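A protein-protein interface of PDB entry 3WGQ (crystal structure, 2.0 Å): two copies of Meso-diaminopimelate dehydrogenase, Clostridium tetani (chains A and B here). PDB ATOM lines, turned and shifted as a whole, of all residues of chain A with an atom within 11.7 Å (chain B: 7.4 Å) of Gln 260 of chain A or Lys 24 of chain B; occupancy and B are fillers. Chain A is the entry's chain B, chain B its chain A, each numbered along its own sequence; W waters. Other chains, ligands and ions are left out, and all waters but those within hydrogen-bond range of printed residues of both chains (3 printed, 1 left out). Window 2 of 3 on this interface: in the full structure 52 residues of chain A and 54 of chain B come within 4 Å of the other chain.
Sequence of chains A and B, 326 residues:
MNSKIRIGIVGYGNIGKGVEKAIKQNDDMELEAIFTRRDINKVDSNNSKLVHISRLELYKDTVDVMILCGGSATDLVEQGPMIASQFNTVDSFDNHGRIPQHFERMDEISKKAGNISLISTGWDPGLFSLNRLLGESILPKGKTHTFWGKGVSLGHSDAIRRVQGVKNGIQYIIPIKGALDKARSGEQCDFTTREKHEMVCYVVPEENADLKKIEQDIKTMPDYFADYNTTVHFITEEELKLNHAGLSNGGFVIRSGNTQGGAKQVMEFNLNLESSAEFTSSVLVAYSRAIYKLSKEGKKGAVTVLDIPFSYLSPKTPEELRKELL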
ATOM      1  N   SER A 137      29.739 -17.590 -31.250  1.00  0.00           N
ATOM      2  CA  SER A 137      29.106 -16.711 -32.231  1.00  0.00           C
ATOM      3  C   SER A 137      27.704 -17.223 -32.579  1.00  0.00           C
ATOM      4  O   SER A 137      26.746 -16.453 -32.647  1.00  0.00           O
ATOM      5  CB  SER A 137      29.944 -16.638 -33.503  1.00  0.00           C
ATOM      6  OG  SER A 137      31.135 -15.917 -33.270  1.00  0.00           O
ATOM      7  N   ILE A 138      27.595 -18.530 -32.795  1.00  0.00           N
ATOM      8  CA  ILE A 138      26.317 -19.147 -33.131  1.00  0.00           C
ATOM      9  C   ILE A 138      25.401 -19.193 -31.906  1.00  0.00           C
ATOM     10  O   ILE A 138      24.194 -18.937 -32.002  1.00  0.00           O
ATOM     11  CB  ILE A 138      26.525 -20.590 -33.648  1.00  0.00           C
ATOM     12  CG1 ILE A 138      27.508 -20.592 -34.825  1.00  0.00           C
ATOM     13  CG2 ILE A 138      25.195 -21.201 -34.025  1.00  0.00           C
ATOM     14  CD1 ILE A 138      27.099 -19.743 -35.990  1.00  0.00           C
ATOM     15  N   LEU A 139      25.984 -19.527 -30.759  1.00  0.00           N
ATOM     16  CA  LEU A 139      25.236 -19.617 -29.508  1.00  0.00           C
ATOM     17  C   LEU A 139      25.813 -18.647 -28.473  1.00  0.00           C
ATOM     18  O   LEU A 139      26.524 -19.050 -27.557  1.00  0.00           O
ATOM     19  CB  LEU A 139      25.288 -21.055 -28.983  1.00  0.00           C
ATOM     20  CG  LEU A 139      24.605 -22.116 -29.853  1.00  0.00           C
ATOM     21  CD1 LEU A 139      24.914 -23.506 -29.295  1.00  0.00           C
ATOM     22  CD2 LEU A 139      23.097 -21.868 -29.891  1.00  0.00           C
ATOM     23  N   PRO A 140      25.492 -17.351 -28.607  1.00  0.00           N
ATOM     24  CA  PRO A 140      25.969 -16.295 -27.705  1.00  0.00           C
ATOM     25  C   PRO A 140      25.647 -16.520 -26.227  1.00  0.00           C
ATOM     26  O   PRO A 140      26.349 -16.024 -25.349  1.00  0.00           O
ATOM     27  CB  PRO A 140      25.302 -15.046 -28.265  1.00  0.00           C
ATOM     28  CG  PRO A 140      24.007 -15.581 -28.798  1.00  0.00           C
ATOM     29  CD  PRO A 140      24.451 -16.831 -29.512  1.00  0.00           C
ATOM     30  N   LYS A 141      24.581 -17.261 -25.956  1.00  0.00           N
ATOM     31  CA  LYS A 141      24.200 -17.557 -24.586  1.00  0.00           C
ATOM     32  C   LYS A 141      24.557 -19.015 -24.326  1.00  0.00           C
ATOM     33  O   LYS A 141      23.907 -19.924 -24.832  1.00  0.00           O
ATOM     34  CB  LYS A 141      22.698 -17.343 -24.384  1.00  0.00           C
ATOM     35  CG  LYS A 141      22.197 -15.945 -24.749  1.00  0.00           C
ATOM     36  CD  LYS A 141      22.874 -14.872 -23.922  1.00  0.00           C
ATOM     37  CE  LYS A 141      22.320 -13.498 -24.255  1.00  0.00           C
ATOM     38  NZ  LYS A 141      23.049 -12.422 -23.519  1.00  0.00           N
ATOM     39  N   GLY A 142      25.611 -19.231 -23.554  1.00  0.00           N
ATOM     40  CA  GLY A 142      26.028 -20.588 -23.256  1.00  0.00           C
ATOM     41  C   GLY A 142      27.453 -20.625 -22.738  1.00  0.00           C
ATOM     42  O   GLY A 142      28.024 -19.580 -22.411  1.00  0.00           O
ATOM     43  N   GLN A 188      24.270 -26.641 -18.724  1.00  0.00           N
ATOM     44  CA  GLN A 188      25.494 -25.852 -18.707  1.00  0.00           C
ATOM     45  C   GLN A 188      25.990 -25.655 -17.278  1.00  0.00           C
ATOM     46  O   GLN A 188      25.204 -25.471 -16.349  1.00  0.00           O
ATOM     47  CB  GLN A 188      25.283 -24.502 -19.412  1.00  0.00           C
ATOM     48  CG  GLN A 188      24.079 -23.697 -18.943  1.00  0.00           C
ATOM     49  CD  GLN A 188      23.747 -22.543 -19.887  1.00  0.00           C
ATOM     50  OE1 GLN A 188      24.560 -21.637 -20.100  1.00  0.00           O
ATOM     51  NE2 GLN A 188      22.546 -22.575 -20.460  1.00  0.00           N
ATOM     52  N   SER A 256      27.957 -25.431 -25.196  1.00  0.00           N
ATOM     53  CA  SER A 256      26.682 -25.846 -24.654  1.00  0.00           C
ATOM     54  C   SER A 256      25.919 -24.553 -24.431  1.00  0.00           C
ATOM     55  O   SER A 256      26.318 -23.708 -23.624  1.00  0.00           O
ATOM     56  CB  SER A 256      26.890 -26.597 -23.333  1.00  0.00           C
ATOM     57  OG  SER A 256      25.660 -27.054 -22.797  1.00  0.00           O
ATOM     58  N   GLY A 257      24.839 -24.380 -25.179  1.00  0.00           N
ATOM     59  CA  GLY A 257      24.066 -23.170 -25.040  1.00  0.00           C
ATOM     60  C   GLY A 257      22.582 -23.427 -24.988  1.00  0.00           C
ATOM     61  O   GLY A 257      22.114 -24.567 -25.040  1.00  0.00           O
ATOM     62  N   ASN A 258      21.833 -22.345 -24.884  1.00  0.00           N
ATOM     63  CA  ASN A 258      20.394 -22.441 -24.834  1.00  0.00           C
ATOM     64  C   ASN A 258      19.819 -21.373 -25.739  1.00  0.00           C
ATOM     65  O   ASN A 258      20.359 -20.272 -25.843  1.00  0.00           O
ATOM     66  CB  ASN A 258      19.903 -22.234 -23.403  1.00  0.00           C
ATOM     67  CG  ASN A 258      20.489 -20.991 -22.769  1.00  0.00           C
ATOM     68  OD1 ASN A 258      21.681 -20.943 -22.458  1.00  0.00           O
ATOM     69  ND2 ASN A 258      19.659 -19.970 -22.587  1.00  0.00           N
ATOM     70  N   THR A 259      18.733 -21.714 -26.414  1.00  0.00           N
ATOM     71  CA  THR A 259      18.059 -20.773 -27.289  1.00  0.00           C
ATOM     72  C   THR A 259      17.076 -20.007 -26.408  1.00  0.00           C
ATOM     73  O   THR A 259      16.738 -20.465 -25.314  1.00  0.00           O
ATOM     74  CB  THR A 259      17.294 -21.524 -28.402  1.00  0.00           C
ATOM     75  OG1 THR A 259      18.192 -21.813 -29.480  1.00  0.00           O
ATOM     76  CG2 THR A 259      16.121 -20.698 -28.911  1.00  0.00           C
ATOM     77  N   GLN A 260      16.645 -18.832 -26.854  1.00  0.00           N
ATOM     78  CA  GLN A 260      15.678 -18.074 -26.079  1.00  0.00           C
ATOM     79  C   GLN A 260      14.513 -19.014 -25.805  1.00  0.00           C
ATOM     80  O   GLN A 260      13.736 -19.333 -26.706  1.00  0.00           O
ATOM     81  CB  GLN A 260      15.188 -16.856 -26.864  1.00  0.00           C
ATOM     82  CG  GLN A 260      16.028 -15.603 -26.667  1.00  0.00           C
ATOM     83  CD  GLN A 260      15.948 -15.058 -25.250  1.00  0.00           C
ATOM     84  OE1 GLN A 260      16.537 -14.023 -24.939  1.00  0.00           O
ATOM     85  NE2 GLN A 260      15.215 -15.753 -24.383  1.00  0.00           N
ATOM     86  N   GLY A 261      14.408 -19.475 -24.565  1.00  0.00           N
ATOM     87  CA  GLY A 261      13.336 -20.388 -24.218  1.00  0.00           C
ATOM     88  C   GLY A 261      13.837 -21.564 -23.406  1.00  0.00           C
ATOM     89  O   GLY A 261      13.041 -22.292 -22.818  1.00  0.00           O
ATOM     90  N   GLY A 262      15.154 -21.760 -23.381  1.00  0.00           N
ATOM     91  CA  GLY A 262      15.726 -22.854 -22.608  1.00  0.00           C
ATOM     92  C   GLY A 262      16.003 -24.145 -23.363  1.00  0.00           C
ATOM     93  O   GLY A 262      16.325 -25.167 -22.757  1.00  0.00           O
ATOM     94  N   ALA A 263      15.866 -24.123 -24.682  1.00  0.00           N
ATOM     95  CA  ALA A 263      16.137 -25.322 -25.468  1.00  0.00           C
ATOM     96  C   ALA A 263      17.650 -25.545 -25.462  1.00  0.00           C
ATOM     97  O   ALA A 263      18.420 -24.607 -25.663  1.00  0.00           O
ATOM     98  CB  ALA A 263      15.631 -25.136 -26.896  1.00  0.00           C
ATOM     99  N   LYS A 264      18.068 -26.785 -25.231  1.00  0.00           N
ATOM    100  CA  LYS A 264      19.490 -27.132 -25.178  1.00  0.00           C
ATOM    101  C   LYS A 264      20.077 -27.354 -26.567  1.00  0.00           C
ATOM    102  O   LYS A 264      19.608 -28.208 -27.316  1.00  0.00           O
ATOM    103  CB  LYS A 264      19.696 -28.406 -24.351  1.00  0.00           C
ATOM    104  CG  LYS A 264      19.172 -28.331 -22.921  1.00  0.00           C
ATOM    105  CD  LYS A 264      19.167 -29.714 -22.285  1.00  0.00           C
ATOM    106  CE  LYS A 264      18.772 -29.654 -20.819  1.00  0.00           C
ATOM    107  NZ  LYS A 264      19.749 -28.863 -20.023  1.00  0.00           N
ATOM    108  N   GLN A 265      21.108 -26.587 -26.903  1.00  0.00           N
ATOM    109  CA  GLN A 265      21.760 -26.715 -28.202  1.00  0.00           C
ATOM    110  C   GLN A 265      23.233 -26.965 -27.916  1.00  0.00           C
ATOM    111  O   GLN A 265      23.879 -26.189 -27.211  1.00  0.00           O
ATOM    112  CB  GLN A 265      21.572 -25.428 -29.014  1.00  0.00           C
ATOM    113  CG  GLN A 265      20.144 -24.881 -28.974  1.00  0.00           C
ATOM    114  CD  GLN A 265      19.173 -25.611 -29.892  1.00  0.00           C
ATOM    115  OE1 GLN A 265      19.120 -26.842 -29.925  1.00  0.00           O
ATOM    116  NE2 GLN A 265      18.388 -24.845 -30.632  1.00  0.00           N
ATOM    117  N   LYS B  17      10.128 -17.413 -36.263  1.00  0.00           N
ATOM    118  CA  LYS B  17       9.893 -17.228 -34.835  1.00  0.00           C
ATOM    119  C   LYS B  17      11.213 -17.389 -34.081  1.00  0.00           C
ATOM    120  O   LYS B  17      11.487 -16.656 -33.131  1.00  0.00           O
ATOM    121  CB  LYS B  17       8.864 -18.241 -34.308  1.00  0.00           C
ATOM    122  CG  LYS B  17       7.427 -17.960 -34.728  1.00  0.00           C
ATOM    123  CD  LYS B  17       6.463 -18.939 -34.051  1.00  0.00           C
ATOM    124  CE  LYS B  17       5.032 -18.750 -34.533  1.00  0.00           C
ATOM    125  NZ  LYS B  17       4.880 -19.088 -35.974  1.00  0.00           N
ATOM    126  N   GLY B  18      12.025 -18.347 -34.516  1.00  0.00           N
ATOM    127  CA  GLY B  18      13.312 -18.567 -33.877  1.00  0.00           C
ATOM    128  C   GLY B  18      14.255 -17.389 -34.071  1.00  0.00           C
ATOM    129  O   GLY B  18      15.055 -17.069 -33.190  1.00  0.00           O
ATOM    130  N   VAL B  19      14.171 -16.747 -35.234  1.00  0.00           N
ATOM    131  CA  VAL B  19      15.023 -15.593 -35.514  1.00  0.00           C
ATOM    132  C   VAL B  19      14.631 -14.432 -34.605  1.00  0.00           C
ATOM    133  O   VAL B  19      15.488 -13.704 -34.101  1.00  0.00           O
ATOM    134  CB  VAL B  19      14.918 -15.156 -37.005  1.00  0.00           C
ATOM    135  CG1 VAL B  19      15.596 -13.803 -37.209  1.00  0.00           C
ATOM    136  CG2 VAL B  19      15.582 -16.202 -37.895  1.00  0.00           C
ATOM    137  N   GLU B  20      13.331 -14.266 -34.390  1.00  0.00           N
ATOM    138  CA  GLU B  20      12.835 -13.203 -33.521  1.00  0.00           C
ATOM    139  C   GLU B  20      13.406 -13.361 -32.112  1.00  0.00           C
ATOM    140  O   GLU B  20      13.804 -12.387 -31.475  1.00  0.00           O
ATOM    141  CB  GLU B  20      11.305 -13.238 -33.481  1.00  0.00           C
ATOM    142  CG  GLU B  20      10.670 -12.331 -32.436  1.00  0.00           C
ATOM    143  CD  GLU B  20       9.161 -12.300 -32.553  1.00  0.00           C
ATOM    144  OE1 GLU B  20       8.555 -13.371 -32.773  1.00  0.00           O
ATOM    145  OE2 GLU B  20       8.578 -11.205 -32.421  1.00  0.00           O
ATOM    146  N   LYS B  21      13.465 -14.591 -31.626  1.00  0.00           N
ATOM    147  CA  LYS B  21      13.993 -14.813 -30.289  1.00  0.00           C
ATOM    148  C   LYS B  21      15.508 -14.676 -30.261  1.00  0.00           C
ATOM    149  O   LYS B  21      16.063 -14.058 -29.355  1.00  0.00           O
ATOM    150  CB  LYS B  21      13.579 -16.190 -29.773  1.00  0.00           C
ATOM    151  CG  LYS B  21      12.113 -16.274 -29.371  1.00  0.00           C
ATOM    152  CD  LYS B  21      11.371 -17.296 -30.215  1.00  0.00           C
ATOM    153  CE  LYS B  21      11.949 -18.689 -30.037  1.00  0.00           C
ATOM    154  NZ  LYS B  21      11.417 -19.641 -31.061  1.00  0.00           N
ATOM    155  N   ALA B  22      16.173 -15.236 -31.264  1.00  0.00           N
ATOM    156  CA  ALA B  22      17.625 -15.165 -31.328  1.00  0.00           C
ATOM    157  C   ALA B  22      18.126 -13.724 -31.398  1.00  0.00           C
ATOM    158  O   ALA B  22      19.181 -13.407 -30.854  1.00  0.00           O
ATOM    159  CB  ALA B  22      18.138 -15.955 -32.526  1.00  0.00           C
ATOM    160  N   ILE B  23      17.382 -12.851 -32.068  1.00  0.00           N
ATOM    161  CA  ILE B  23      17.814 -11.468 -32.181  1.00  0.00           C
ATOM    162  C   ILE B  23      17.915 -10.867 -30.789  1.00  0.00           C
ATOM    163  O   ILE B  23      18.780 -10.037 -30.518  1.00  0.00           O
ATOM    164  CB  ILE B  23      16.846 -10.636 -33.055  1.00  0.00           C
ATOM    165  CG1 ILE B  23      16.950 -11.098 -34.509  1.00  0.00           C
ATOM    166  CG2 ILE B  23      17.188  -9.153 -32.959  1.00  0.00           C
ATOM    167  CD1 ILE B  23      16.100 -10.302 -35.473  1.00  0.00           C
ATOM    168  N   LYS B  24      17.045 -11.327 -29.899  1.00  0.00           N
ATOM    169  CA  LYS B  24      17.032 -10.840 -28.535  1.00  0.00           C
ATOM    170  C   LYS B  24      18.294 -11.241 -27.774  1.00  0.00           C
ATOM    171  O   LYS B  24      18.628 -10.627 -26.764  1.00  0.00           O
ATOM    172  CB  LYS B  24      15.788 -11.363 -27.812  1.00  0.00           C
ATOM    173  CG  LYS B  24      14.480 -10.925 -28.458  1.00  0.00           C
ATOM    174  CD  LYS B  24      13.271 -11.470 -27.706  1.00  0.00           C
ATOM    175  CE  LYS B  24      11.968 -11.021 -28.357  1.00  0.00           C
ATOM    176  NZ  LYS B  24      10.766 -11.591 -27.678  1.00  0.00           N
ATOM    177  N   GLN B  25      18.994 -12.268 -28.253  1.00  0.00           N
ATOM    178  CA  GLN B  25      20.222 -12.717 -27.598  1.00  0.00           C
ATOM    179  C   GLN B  25      21.434 -11.968 -28.145  1.00  0.00           C
ATOM    180  O   GLN B  25      22.571 -12.258 -27.773  1.00  0.00           O
ATOM    181  CB  GLN B  25      20.432 -14.227 -27.804  1.00  0.00           C
ATOM    182  CG  GLN B  25      19.390 -15.125 -27.153  1.00  0.00           C
ATOM    183  CD  GLN B  25      19.772 -16.603 -27.205  1.00  0.00           C
ATOM    184  OE1 GLN B  25      20.157 -17.119 -28.253  1.00  0.00           O
ATOM    185  NE2 GLN B  25      19.657 -17.287 -26.072  1.00  0.00           N
ATOM    186  N   ASN B  26      21.187 -11.007 -29.030  1.00  0.00           N
ATOM    187  CA  ASN B  26      22.258 -10.218 -29.645  1.00  0.00           C
ATOM    188  C   ASN B  26      22.041  -8.719 -29.455  1.00  0.00           C
ATOM    189  O   ASN B  26      21.183  -8.119 -30.101  1.00  0.00           O
ATOM    190  CB  ASN B  26      22.339 -10.535 -31.141  1.00  0.00           C
ATOM    191  CG  ASN B  26      22.760 -11.963 -31.410  1.00  0.00           C
ATOM    192  OD1 ASN B  26      23.937 -12.245 -31.613  1.00  0.00           O
ATOM    193  ND2 ASN B  26      21.793 -12.878 -31.404  1.00  0.00           N
ATOM    194  N   ASP B  27      22.844  -8.121 -28.580  1.00  0.00           N
ATOM    195  CA  ASP B  27      22.756  -6.699 -28.264  1.00  0.00           C
ATOM    196  C   ASP B  27      22.961  -5.741 -29.429  1.00  0.00           C
ATOM    197  O   ASP B  27      22.348  -4.677 -29.469  1.00  0.00           O
ATOM    198  CB  ASP B  27      23.767  -6.345 -27.168  1.00  0.00           C
ATOM    199  CG  ASP B  27      23.479  -7.046 -25.861  1.00  0.00           C
ATOM    200  OD1 ASP B  27      22.400  -6.799 -25.277  1.00  0.00           O
ATOM    201  OD2 ASP B  27      24.331  -7.848 -25.417  1.00  0.00           O
ATOM    202  N   MET B  29      21.905  -5.943 -32.300  1.00  0.00           N
ATOM    203  CA  MET B  29      20.847  -6.081 -33.296  1.00  0.00           C
ATOM    204  C   MET B  29      19.451  -5.658 -32.888  1.00  0.00           C
ATOM    205  O   MET B  29      19.072  -5.733 -31.728  1.00  0.00           O
ATOM    206  CB  MET B  29      20.802  -7.508 -33.809  1.00  0.00           C
ATOM    207  CG  MET B  29      21.884  -7.793 -34.820  1.00  0.00           C
ATOM    208  SD  MET B  29      21.783  -9.464 -35.354  1.00  0.00           S
ATOM    209  CE  MET B  29      23.510  -9.805 -35.748  1.00  0.00           C
ATOM    210  N   LEU B  31      15.207  -5.703 -34.366  1.00  0.00           N
ATOM    211  CA  LEU B  31      14.217  -6.227 -35.294  1.00  0.00           C
ATOM    212  C   LEU B  31      13.324  -5.093 -35.797  1.00  0.00           C
ATOM    213  O   LEU B  31      12.581  -4.489 -35.017  1.00  0.00           O
ATOM    214  CB  LEU B  31      13.362  -7.293 -34.599  1.00  0.00           C
ATOM    215  CG  LEU B  31      12.219  -7.916 -35.402  1.00  0.00           C
ATOM    216  CD1 LEU B  31      12.729  -8.444 -36.730  1.00  0.00           C
ATOM    217  CD2 LEU B  31      11.595  -9.036 -34.588  1.00  0.00           C
ATOM    218  N   LYS B  49       4.820  -5.649 -34.588  1.00  0.00           N
ATOM    219  CA  LYS B  49       5.827  -6.498 -35.225  1.00  0.00           C
ATOM    220  C   LYS B  49       5.480  -7.077 -36.592  1.00  0.00           C
ATOM    221  O   LYS B  49       6.242  -6.908 -37.546  1.00  0.00           O
ATOM    222  CB  LYS B  49       6.241  -7.626 -34.277  1.00  0.00           C
ATOM    223  CG  LYS B  49       7.748  -7.656 -34.013  1.00  0.00           C
ATOM    224  CD  LYS B  49       8.255  -6.301 -33.507  1.00  0.00           C
ATOM    225  CE  LYS B  49       9.742  -6.342 -33.182  1.00  0.00           C
ATOM    226  NZ  LYS B  49      10.252  -5.049 -32.640  1.00  0.00           N
ATOM    227  N   GLU B 278      15.298 -23.471 -34.084  1.00  0.00           N
ATOM    228  CA  GLU B 278      15.880 -22.341 -33.362  1.00  0.00           C
ATOM    229  C   GLU B 278      17.389 -22.276 -33.525  1.00  0.00           C
ATOM    230  O   GLU B 278      17.968 -21.198 -33.433  1.00  0.00           O
ATOM    231  CB  GLU B 278      15.519 -22.391 -31.878  1.00  0.00           C
ATOM    232  CG  GLU B 278      14.018 -22.307 -31.637  1.00  0.00           C
ATOM    233  CD  GLU B 278      13.664 -22.244 -30.171  1.00  0.00           C
ATOM    234  OE1 GLU B 278      14.331 -22.920 -29.365  1.00  0.00           O
ATOM    235  OE2 GLU B 278      12.707 -21.528 -29.823  1.00  0.00           O
ATOM    236  N   SER B 282      19.559 -19.194 -35.027  1.00  0.00           N
ATOM    237  CA  SER B 282      20.749 -18.584 -34.428  1.00  0.00           C
ATOM    238  C   SER B 282      21.861 -18.476 -35.474  1.00  0.00           C
ATOM    239  O   SER B 282      22.592 -17.490 -35.514  1.00  0.00           O
ATOM    240  CB  SER B 282      21.254 -19.428 -33.254  1.00  0.00           C
ATOM    241  OG  SER B 282      20.217 -19.698 -32.335  1.00  0.00           O
ATOM    242  N   VAL B 285      21.147 -15.544 -37.775  1.00  0.00           N
ATOM    243  CA  VAL B 285      21.403 -14.255 -37.148  1.00  0.00           C
ATOM    244  C   VAL B 285      22.901 -13.943 -37.075  1.00  0.00           C
ATOM    245  O   VAL B 285      23.321 -12.834 -37.402  1.00  0.00           O
ATOM    246  CB  VAL B 285      20.775 -14.190 -35.733  1.00  0.00           C
ATOM    247  CG1 VAL B 285      21.198 -12.904 -35.029  1.00  0.00           C
ATOM    248  CG2 VAL B 285      19.252 -14.242 -35.849  1.00  0.00           C
HETATM  249  O   HOH W   1      17.592 -18.077 -29.390  1.00  0.00           O
HETATM  250  O   HOH W   2      22.597 -18.779 -27.433  1.00  0.00           O
HETATM  251  O   HOH W   3      20.596 -10.737 -24.468  1.00  0.00           O
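OE2 of Glu 278 of chain B lies within salt-bridge range of NZ of Lys 21 of chain B, 2.6 Å away.
The backbone carbonyl oxygen (O) of Glu 278 of chain B lies within hydrogen-bond range of the side-chain hydroxyl (OG) of Ser 282 of chain B (2.9 Å).
O of Lys 141 of chain A sits at hydrogen-bond distance from N of Asn 258 of chain A (3.2 Å).
OD1 of Asn 258 of chain A is in hydrogen-bond range of NE2 of Gln 188 of chain A.
The backbone NH of Gly 257 of chain A is in hydrogen-bond range of the backbone carbonyl oxygen of Gln 265 of chain A, 2.9 Å away.
The side-chain amide nitrogen (NE2) of Gln 265 of chain A lies within hydrogen-bond range of the side-chain hydroxyl (OG1) of Thr 259 of chain A, at 3.2 Å.
Of the 17 printed residues of chain B, 5 touch a printed residue of chain A.
Among the printed residues, 12 pairs touch across the chains.
The backbone carbonyl oxygen (O) of Asn 258 of chain A sits at hydrogen-bond distance from the side-chain amide nitrogen (NE2) of Gln 25 of chain B.
The backbone NH (N) of Gln 260 of chain A lies close to the side-chain amide nitrogen (NE2) of Gln 25 of chain B, 3.5 Å away.
Ile 138 of chain A touches Ser 282 of chain B.
O of Gln 25 of chain B touches CG of Pro 140 of chain A, 3.8 Å away.
Lys 141 of chain A touches Gln 25 of chain B.
NE2 of Gln 25 of chain B touches C of Thr 259 of chain A (3.8 Å).
Thr 259 of chain A touches Glu 278 of chain B (CG2 to OE1, 2.9 Å).
O of Lys 21 of chain B touches CG of Gln 260 of chain A, 3.1 Å away.
Gln 260 of chain A touches Lys 24 of chain B (OE1 to CB, 3.99 Å).
Gln 260 of chain A touches Glu 278 of chain B (O to OE2, 3.9 Å).
Ala 263 of chain A touches Glu 278 of chain B (CB to OE1, 3.6 Å).
CB of Glu 278 of chain B touches NE2 of Gln 265 of chain A, at 3.98 Å.
Water W1 lies within hydrogen-bond range of N of Gln 260 of chain A and OE1 of Gln 25 of chain B.
Water W2 lies within hydrogen-bond range of the backbone NH of Lys 141 of chain A (2.9 Å), the side-chain amide oxygen of Gln 25 of chain B (3.1 Å) and the backbone carbonyl oxygen of Asn 258 of chain A (3.1 Å).
Water W3 bridges O of Lys 24 of chain B and NZ of Lys 141 of chain A.
No position is printed for both chains.
Printed residues of chain B within 4 Å of Pro 140 of chain A: Gln 25.
Val 19 of chain B touches none of the printed residues of chain A.
No residue of chain A comes within 4 Å of Glu 20 of chain B.
No residue of chain A comes within 4 Å of Ile 23 of chain B.
No residue of chain A comes within 4 Å of Asn 26 of chain B.
No residue of chain A comes within 4 Å of Asp 27 of chain B.
Of the printed residues of chain A, Glu 278 of chain B touches Thr 259, Gln 260, Ala 263 and Gln 265.
The nearest printed residue of chain A that does not touch Lys 24 of chain B is Lys 141 of chain A (5.3 Å).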
